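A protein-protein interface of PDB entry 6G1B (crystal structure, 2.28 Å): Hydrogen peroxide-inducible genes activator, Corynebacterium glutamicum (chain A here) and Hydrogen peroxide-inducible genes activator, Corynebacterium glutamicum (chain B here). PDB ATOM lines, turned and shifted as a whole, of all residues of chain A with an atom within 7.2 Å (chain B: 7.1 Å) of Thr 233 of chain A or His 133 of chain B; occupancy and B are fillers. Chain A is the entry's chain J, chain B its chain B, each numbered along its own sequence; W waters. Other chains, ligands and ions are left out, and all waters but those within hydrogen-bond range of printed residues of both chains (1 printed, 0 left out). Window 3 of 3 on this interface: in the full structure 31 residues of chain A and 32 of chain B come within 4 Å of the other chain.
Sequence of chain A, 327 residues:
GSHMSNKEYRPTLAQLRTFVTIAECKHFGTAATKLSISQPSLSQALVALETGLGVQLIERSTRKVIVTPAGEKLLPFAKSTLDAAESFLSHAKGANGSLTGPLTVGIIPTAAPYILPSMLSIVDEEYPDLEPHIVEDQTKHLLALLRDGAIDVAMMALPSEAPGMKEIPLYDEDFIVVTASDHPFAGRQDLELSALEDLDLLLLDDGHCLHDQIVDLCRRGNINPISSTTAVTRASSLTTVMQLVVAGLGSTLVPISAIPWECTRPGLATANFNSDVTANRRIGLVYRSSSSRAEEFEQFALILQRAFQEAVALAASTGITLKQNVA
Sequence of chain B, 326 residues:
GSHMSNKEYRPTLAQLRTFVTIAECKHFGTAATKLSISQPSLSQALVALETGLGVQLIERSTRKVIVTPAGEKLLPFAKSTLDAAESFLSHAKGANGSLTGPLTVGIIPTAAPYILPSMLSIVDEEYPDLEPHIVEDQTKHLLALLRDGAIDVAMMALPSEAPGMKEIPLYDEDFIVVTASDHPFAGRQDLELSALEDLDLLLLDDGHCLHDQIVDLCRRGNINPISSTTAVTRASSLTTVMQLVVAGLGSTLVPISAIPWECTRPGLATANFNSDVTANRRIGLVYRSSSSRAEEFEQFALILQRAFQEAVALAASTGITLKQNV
The backbone carbonyl oxygen (O) of Ala 231 of chain A sits at hydrogen-bond distance from the backbone NH (N) of Ile 134 of chain B (2.7 Å). N of Thr 233 of chain A sits at hydrogen-bond distance from O of Ile 134 of chain B (2.8 Å). The backbone carbonyl oxygen of Arg 234 of chain A sits at hydrogen-bond distance from the backbone NH of Glu 136 of chain B.
N of His 133 of chain B lies within hydrogen-bond range of O of Leu 103 of chain B (2.8 Å). The backbone NH (N) of Val 105 of chain B is in hydrogen-bond range of the backbone carbonyl oxygen (O) of His 133 of chain B. N of Val 135 of chain B sits at hydrogen-bond distance from O of Val 105 of chain B (2.9 Å). OE2 of Glu 131 of chain B lies within hydrogen-bond range of NE2 of His 133 of chain B, at 3.3 Å.
Leu 120 of chain B touches Ala 231 of chain A. O of Ala 231 of chain A touches O of Pro 132 of chain B (3.7 Å). Ala 231 of chain A touches His 133 of chain B. CA of Val 232 of chain A touches O of Ile 134 of chain B, 3.4 Å away. His 133 of chain B touches Thr 233 of chain A (CB to OG1, 3.8 Å). N of Arg 234 of chain A touches O of Ile 134 of chain B, at 3.6 Å. O of Arg 234 of chain A touches CA of Val 135 of chain B, 3.6 Å away. Ala 235 of chain A touches Glu 136 of chain B (C to O, 3.6 Å).
Of chain B, only His 133 and Ile 134 come within 4 Å of Thr 233 of chain A. Printed residues of chain A within 4 Å of Leu 120 of chain B: Ala 231. Of the printed residues of chain A, Pro 132 of chain B touches Ala 231 (3.7 Å). His 133 of chain B touches two residues of chain A. Printed residues of chain A within 4 Å of Val 135 of chain B: Arg 234.
Of the 16 printed residues of chain B, 6 touch a printed residue of chain A. Hydrophobic or aromatic side chains of chain B that line the printed part of chain A: Leu 120, His 133 and Ile 134. Among the printed residues, no Asp or Glu carboxylate lies within 4 Å of a Lys or Arg side-chain nitrogen of the other chain.
Water W1 bridges O of Glu 136 of chain B (3.0 Å) and NH1 of Arg 234 of chain A (3.3 Å).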
ATOM      1  N   LEU A 201      -6.435  34.321  31.397  1.00  0.00           N
ATOM      2  CA  LEU A 201      -5.133  34.498  32.023  1.00  0.00           C
ATOM      3  C   LEU A 201      -4.031  33.809  31.223  1.00  0.00           C
ATOM      4  O   LEU A 201      -4.186  32.652  30.845  1.00  0.00           O
ATOM      5  CB  LEU A 201      -5.117  34.039  33.482  1.00  0.00           C
ATOM      6  CG  LEU A 201      -5.684  35.073  34.489  1.00  0.00           C
ATOM      7  CD1 LEU A 201      -5.754  34.440  35.872  1.00  0.00           C
ATOM      8  CD2 LEU A 201      -4.936  36.416  34.524  1.00  0.00           C
ATOM      9  N   LEU A 202      -2.960  34.537  30.931  1.00  0.00           N
ATOM     10  CA  LEU A 202      -1.736  33.905  30.483  1.00  0.00           C
ATOM     11  C   LEU A 202      -0.760  34.152  31.594  1.00  0.00           C
ATOM     12  O   LEU A 202      -0.390  35.288  31.832  1.00  0.00           O
ATOM     13  CB  LEU A 202      -1.260  34.459  29.134  1.00  0.00           C
ATOM     14  CG  LEU A 202      -0.001  33.851  28.502  1.00  0.00           C
ATOM     15  CD1 LEU A 202       0.054  32.320  28.555  1.00  0.00           C
ATOM     16  CD2 LEU A 202       0.154  34.344  27.067  1.00  0.00           C
ATOM     17  N   LEU A 203      -0.347  33.092  32.278  1.00  0.00           N
ATOM     18  CA  LEU A 203       0.550  33.205  33.420  1.00  0.00           C
ATOM     19  C   LEU A 203       1.906  32.645  33.078  1.00  0.00           C
ATOM     20  O   LEU A 203       2.004  31.747  32.275  1.00  0.00           O
ATOM     21  CB  LEU A 203      -0.026  32.437  34.600  1.00  0.00           C
ATOM     22  CG  LEU A 203      -1.356  32.965  35.150  1.00  0.00           C
ATOM     23  CD1 LEU A 203      -1.844  32.046  36.259  1.00  0.00           C
ATOM     24  CD2 LEU A 203      -1.226  34.408  35.645  1.00  0.00           C
ATOM     25  N   THR A 230      -5.915  30.892  25.480  1.00  0.00           N
ATOM     26  CA  THR A 230      -5.488  31.758  24.391  1.00  0.00           C
ATOM     27  C   THR A 230      -4.775  30.929  23.313  1.00  0.00           C
ATOM     28  O   THR A 230      -4.515  29.743  23.514  1.00  0.00           O
ATOM     29  CB  THR A 230      -4.570  32.841  24.933  1.00  0.00           C
ATOM     30  N   ALA A 231      -4.449  31.546  22.177  1.00  0.00           N
ATOM     31  CA  ALA A 231      -3.626  30.901  21.147  1.00  0.00           C
ATOM     32  C   ALA A 231      -2.221  30.524  21.653  1.00  0.00           C
ATOM     33  O   ALA A 231      -1.588  29.616  21.115  1.00  0.00           O
ATOM     34  CB  ALA A 231      -3.497  31.799  19.922  1.00  0.00           C
ATOM     35  N   VAL A 232      -1.729  31.256  22.660  1.00  0.00           N
ATOM     36  CA  VAL A 232      -0.445  30.973  23.299  1.00  0.00           C
ATOM     37  C   VAL A 232      -0.603  30.050  24.496  1.00  0.00           C
ATOM     38  O   VAL A 232      -0.951  30.501  25.587  1.00  0.00           O
ATOM     39  CB  VAL A 232       0.261  32.280  23.708  1.00  0.00           C
ATOM     40  CG1 VAL A 232       1.581  32.005  24.429  1.00  0.00           C
ATOM     41  CG2 VAL A 232       0.470  33.123  22.460  1.00  0.00           C
ATOM     42  N   THR A 233      -0.337  28.773  24.264  1.00  0.00           N
ATOM     43  CA  THR A 233      -0.284  27.741  25.299  1.00  0.00           C
ATOM     44  C   THR A 233       0.591  28.103  26.493  1.00  0.00           C
ATOM     45  O   THR A 233       0.150  27.952  27.619  1.00  0.00           O
ATOM     46  CB  THR A 233       0.281  26.425  24.713  1.00  0.00           C
ATOM     47  OG1 THR A 233      -0.413  26.105  23.509  1.00  0.00           O
ATOM     48  CG2 THR A 233       0.185  25.278  25.719  1.00  0.00           C
ATOM     49  N   ARG A 234       1.808  28.582  26.238  1.00  0.00           N
ATOM     50  CA  ARG A 234       2.718  28.992  27.294  1.00  0.00           C
ATOM     51  C   ARG A 234       3.858  29.859  26.753  1.00  0.00           C
ATOM     52  O   ARG A 234       4.406  29.611  25.683  1.00  0.00           O
ATOM     53  CB  ARG A 234       3.291  27.798  28.101  1.00  0.00           C
ATOM     54  CG  ARG A 234       4.098  26.757  27.360  1.00  0.00           C
ATOM     55  CD  ARG A 234       4.779  25.824  28.369  1.00  0.00           C
ATOM     56  NE  ARG A 234       5.068  24.498  27.803  1.00  0.00           N
ATOM     57  CZ  ARG A 234       6.257  24.060  27.379  1.00  0.00           C
ATOM     58  NH1 ARG A 234       7.355  24.832  27.421  1.00  0.00           N
ATOM     59  NH2 ARG A 234       6.341  22.822  26.902  1.00  0.00           N
ATOM     60  N   ALA A 235       4.187  30.895  27.523  1.00  0.00           N
ATOM     61  CA  ALA A 235       5.266  31.807  27.261  1.00  0.00           C
ATOM     62  C   ALA A 235       6.316  31.645  28.345  1.00  0.00           C
ATOM     63  O   ALA A 235       6.023  31.294  29.448  1.00  0.00           O
ATOM     64  CB  ALA A 235       4.699  33.219  27.265  1.00  0.00           C
ATOM     65  N   GLY B 101      -7.073  22.924  10.760  1.00  0.00           N
ATOM     66  CA  GLY B 101      -6.854  22.119  11.933  1.00  0.00           C
ATOM     67  C   GLY B 101      -5.798  22.671  12.881  1.00  0.00           C
ATOM     68  O   GLY B 101      -5.320  23.813  12.737  1.00  0.00           O
ATOM     69  N   PRO B 102      -5.412  21.840  13.869  1.00  0.00           N
ATOM     70  CA  PRO B 102      -4.435  22.264  14.871  1.00  0.00           C
ATOM     71  C   PRO B 102      -3.041  22.426  14.278  1.00  0.00           C
ATOM     72  O   PRO B 102      -2.609  21.593  13.484  1.00  0.00           O
ATOM     73  CB  PRO B 102      -4.465  21.125  15.907  1.00  0.00           C
ATOM     74  CG  PRO B 102      -5.621  20.256  15.542  1.00  0.00           C
ATOM     75  CD  PRO B 102      -5.859  20.451  14.092  1.00  0.00           C
ATOM     76  N   LEU B 103      -2.368  23.511  14.635  1.00  0.00           N
ATOM     77  CA  LEU B 103      -0.967  23.699  14.278  1.00  0.00           C
ATOM     78  C   LEU B 103      -0.263  24.233  15.498  1.00  0.00           C
ATOM     79  O   LEU B 103      -0.536  25.343  15.931  1.00  0.00           O
ATOM     80  CB  LEU B 103      -0.804  24.656  13.096  1.00  0.00           C
ATOM     81  CG  LEU B 103       0.633  24.897  12.622  1.00  0.00           C
ATOM     82  CD1 LEU B 103       1.240  23.582  12.083  1.00  0.00           C
ATOM     83  CD2 LEU B 103       0.672  25.977  11.560  1.00  0.00           C
ATOM     84  N   THR B 104       0.630  23.439  16.074  1.00  0.00           N
ATOM     85  CA  THR B 104       1.375  23.868  17.248  1.00  0.00           C
ATOM     86  C   THR B 104       2.791  24.387  16.857  1.00  0.00           C
ATOM     87  O   THR B 104       3.601  23.650  16.269  1.00  0.00           O
ATOM     88  CB  THR B 104       1.398  22.737  18.267  1.00  0.00           C
ATOM     89  OG1 THR B 104       0.040  22.386  18.575  1.00  0.00           O
ATOM     90  CG2 THR B 104       2.068  23.167  19.534  1.00  0.00           C
ATOM     91  N   VAL B 105       3.048  25.661  17.155  1.00  0.00           N
ATOM     92  CA  VAL B 105       4.253  26.371  16.707  1.00  0.00           C
ATOM     93  C   VAL B 105       5.127  26.776  17.889  1.00  0.00           C
ATOM     94  O   VAL B 105       4.664  27.495  18.783  1.00  0.00           O
ATOM     95  CB  VAL B 105       3.874  27.643  15.898  1.00  0.00           C
ATOM     96  CG1 VAL B 105       5.108  28.219  15.195  1.00  0.00           C
ATOM     97  CG2 VAL B 105       2.778  27.334  14.866  1.00  0.00           C
ATOM     98  N   GLY B 106       6.377  26.318  17.914  1.00  0.00           N
ATOM     99  CA  GLY B 106       7.384  26.826  18.880  1.00  0.00           C
ATOM    100  C   GLY B 106       8.056  28.062  18.313  1.00  0.00           C
ATOM    101  O   GLY B 106       8.348  28.091  17.134  1.00  0.00           O
ATOM    102  N   LEU B 120      -1.037  36.173  14.305  1.00  0.00           N
ATOM    103  CA  LEU B 120      -2.355  35.743  14.803  1.00  0.00           C
ATOM    104  C   LEU B 120      -3.497  36.475  14.116  1.00  0.00           C
ATOM    105  O   LEU B 120      -4.526  35.869  13.857  1.00  0.00           O
ATOM    106  CB  LEU B 120      -2.483  35.912  16.326  1.00  0.00           C
ATOM    107  CG  LEU B 120      -1.626  34.962  17.163  1.00  0.00           C
ATOM    108  CD1 LEU B 120      -1.761  35.332  18.637  1.00  0.00           C
ATOM    109  CD2 LEU B 120      -1.932  33.485  16.932  1.00  0.00           C
ATOM    110  N   GLU B 131      -6.081  26.386  13.519  1.00  0.00           N
ATOM    111  CA  GLU B 131      -6.224  26.468  14.959  1.00  0.00           C
ATOM    112  C   GLU B 131      -4.803  26.533  15.543  1.00  0.00           C
ATOM    113  O   GLU B 131      -4.182  25.504  15.838  1.00  0.00           O
ATOM    114  CB  GLU B 131      -7.008  25.240  15.419  1.00  0.00           C
ATOM    115  CG  GLU B 131      -7.346  25.123  16.897  1.00  0.00           C
ATOM    116  CD  GLU B 131      -8.068  23.805  17.200  1.00  0.00           C
ATOM    117  OE1 GLU B 131      -9.037  23.478  16.460  1.00  0.00           O
ATOM    118  OE2 GLU B 131      -7.647  23.099  18.160  1.00  0.00           O
ATOM    119  N   PRO B 132      -4.242  27.750  15.650  1.00  0.00           N
ATOM    120  CA  PRO B 132      -2.833  27.869  16.033  1.00  0.00           C
ATOM    121  C   PRO B 132      -2.630  27.689  17.529  1.00  0.00           C
ATOM    122  O   PRO B 132      -3.460  28.150  18.314  1.00  0.00           O
ATOM    123  CB  PRO B 132      -2.465  29.280  15.595  1.00  0.00           C
ATOM    124  CG  PRO B 132      -3.736  30.022  15.685  1.00  0.00           C
ATOM    125  CD  PRO B 132      -4.867  29.065  15.432  1.00  0.00           C
ATOM    126  N   HIS B 133      -1.556  26.997  17.912  1.00  0.00           N
ATOM    127  CA  HIS B 133      -1.137  26.900  19.317  1.00  0.00           C
ATOM    128  C   HIS B 133       0.319  27.296  19.404  1.00  0.00           C
ATOM    129  O   HIS B 133       1.144  26.693  18.749  1.00  0.00           O
ATOM    130  CB  HIS B 133      -1.364  25.496  19.852  1.00  0.00           C
ATOM    131  CG  HIS B 133      -2.793  25.077  19.791  1.00  0.00           C
ATOM    132  ND1 HIS B 133      -3.743  25.569  20.659  1.00  0.00           N
ATOM    133  CD2 HIS B 133      -3.453  24.274  18.924  1.00  0.00           C
ATOM    134  CE1 HIS B 133      -4.920  25.064  20.345  1.00  0.00           C
ATOM    135  NE2 HIS B 133      -4.769  24.259  19.308  1.00  0.00           N
ATOM    136  N   ILE B 134       0.629  28.309  20.200  1.00  0.00           N
ATOM    137  CA  ILE B 134       1.971  28.869  20.264  1.00  0.00           C
ATOM    138  C   ILE B 134       2.622  28.530  21.594  1.00  0.00           C
ATOM    139  O   ILE B 134       2.023  28.701  22.670  1.00  0.00           O
ATOM    140  CB  ILE B 134       1.964  30.406  20.121  1.00  0.00           C
ATOM    141  CG1 ILE B 134       1.084  30.856  18.944  1.00  0.00           C
ATOM    142  CG2 ILE B 134       3.373  30.952  20.004  1.00  0.00           C
ATOM    143  CD1 ILE B 134       1.596  30.396  17.593  1.00  0.00           C
ATOM    144  N   VAL B 135       3.852  28.042  21.497  1.00  0.00           N
ATOM    145  CA  VAL B 135       4.723  27.759  22.622  1.00  0.00           C
ATOM    146  C   VAL B 135       5.944  28.655  22.424  1.00  0.00           C
ATOM    147  O   VAL B 135       6.619  28.556  21.414  1.00  0.00           O
ATOM    148  CB  VAL B 135       5.156  26.273  22.662  1.00  0.00           C
ATOM    149  CG1 VAL B 135       6.192  26.038  23.759  1.00  0.00           C
ATOM    150  CG2 VAL B 135       3.958  25.362  22.853  1.00  0.00           C
ATOM    151  N   GLU B 136       6.193  29.547  23.374  1.00  0.00           N
ATOM    152  CA  GLU B 136       7.340  30.423  23.334  1.00  0.00           C
ATOM    153  C   GLU B 136       8.309  29.960  24.418  1.00  0.00           C
ATOM    154  O   GLU B 136       7.945  29.940  25.613  1.00  0.00           O
ATOM    155  CB  GLU B 136       6.941  31.881  23.540  1.00  0.00           C
ATOM    156  CG  GLU B 136       8.102  32.864  23.518  1.00  0.00           C
ATOM    157  CD  GLU B 136       8.462  33.337  24.908  1.00  0.00           C
ATOM    158  OE1 GLU B 136       7.694  34.146  25.452  1.00  0.00           O
ATOM    159  OE2 GLU B 136       9.492  32.872  25.475  1.00  0.00           O
ATOM    160  N   ILE B 151       5.436  19.810  19.676  1.00  0.00           N
ATOM    161  CA  ILE B 151       5.148  20.865  18.684  1.00  0.00           C
ATOM    162  C   ILE B 151       5.360  20.311  17.277  1.00  0.00           C
ATOM    163  O   ILE B 151       6.012  19.278  17.117  1.00  0.00           O
ATOM    164  CB  ILE B 151       5.971  22.152  18.902  1.00  0.00           C
ATOM    165  CG1 ILE B 151       7.449  21.946  18.617  1.00  0.00           C
ATOM    166  CG2 ILE B 151       5.757  22.680  20.330  1.00  0.00           C
ATOM    167  CD1 ILE B 151       8.292  23.177  18.849  1.00  0.00           C
ATOM    168  N   ASP B 152       4.786  20.980  16.282  1.00  0.00           N
ATOM    169  CA  ASP B 152       4.842  20.530  14.888  1.00  0.00           C
ATOM    170  C   ASP B 152       5.994  21.204  14.111  1.00  0.00           C
ATOM    171  O   ASP B 152       6.603  20.612  13.226  1.00  0.00           O
ATOM    172  CB  ASP B 152       3.520  20.823  14.167  1.00  0.00           C
ATOM    173  CG  ASP B 152       2.303  20.208  14.851  1.00  0.00           C
ATOM    174  OD1 ASP B 152       1.286  20.902  14.874  1.00  0.00           O
ATOM    175  OD2 ASP B 152       2.322  19.066  15.355  1.00  0.00           O
ATOM    176  N   VAL B 153       6.242  22.462  14.456  1.00  0.00           N
ATOM    177  CA  VAL B 153       7.241  23.295  13.823  1.00  0.00           C
ATOM    178  C   VAL B 153       7.823  24.261  14.856  1.00  0.00           C
ATOM    179  O   VAL B 153       7.140  24.676  15.777  1.00  0.00           O
ATOM    180  CB  VAL B 153       6.674  24.076  12.625  1.00  0.00           C
ATOM    181  CG1 VAL B 153       6.317  23.149  11.516  1.00  0.00           C
ATOM    182  CG2 VAL B 153       5.441  24.891  13.017  1.00  0.00           C
HETATM  183  O   HOH W   1       7.274  28.065  27.881  1.00  0.00           O
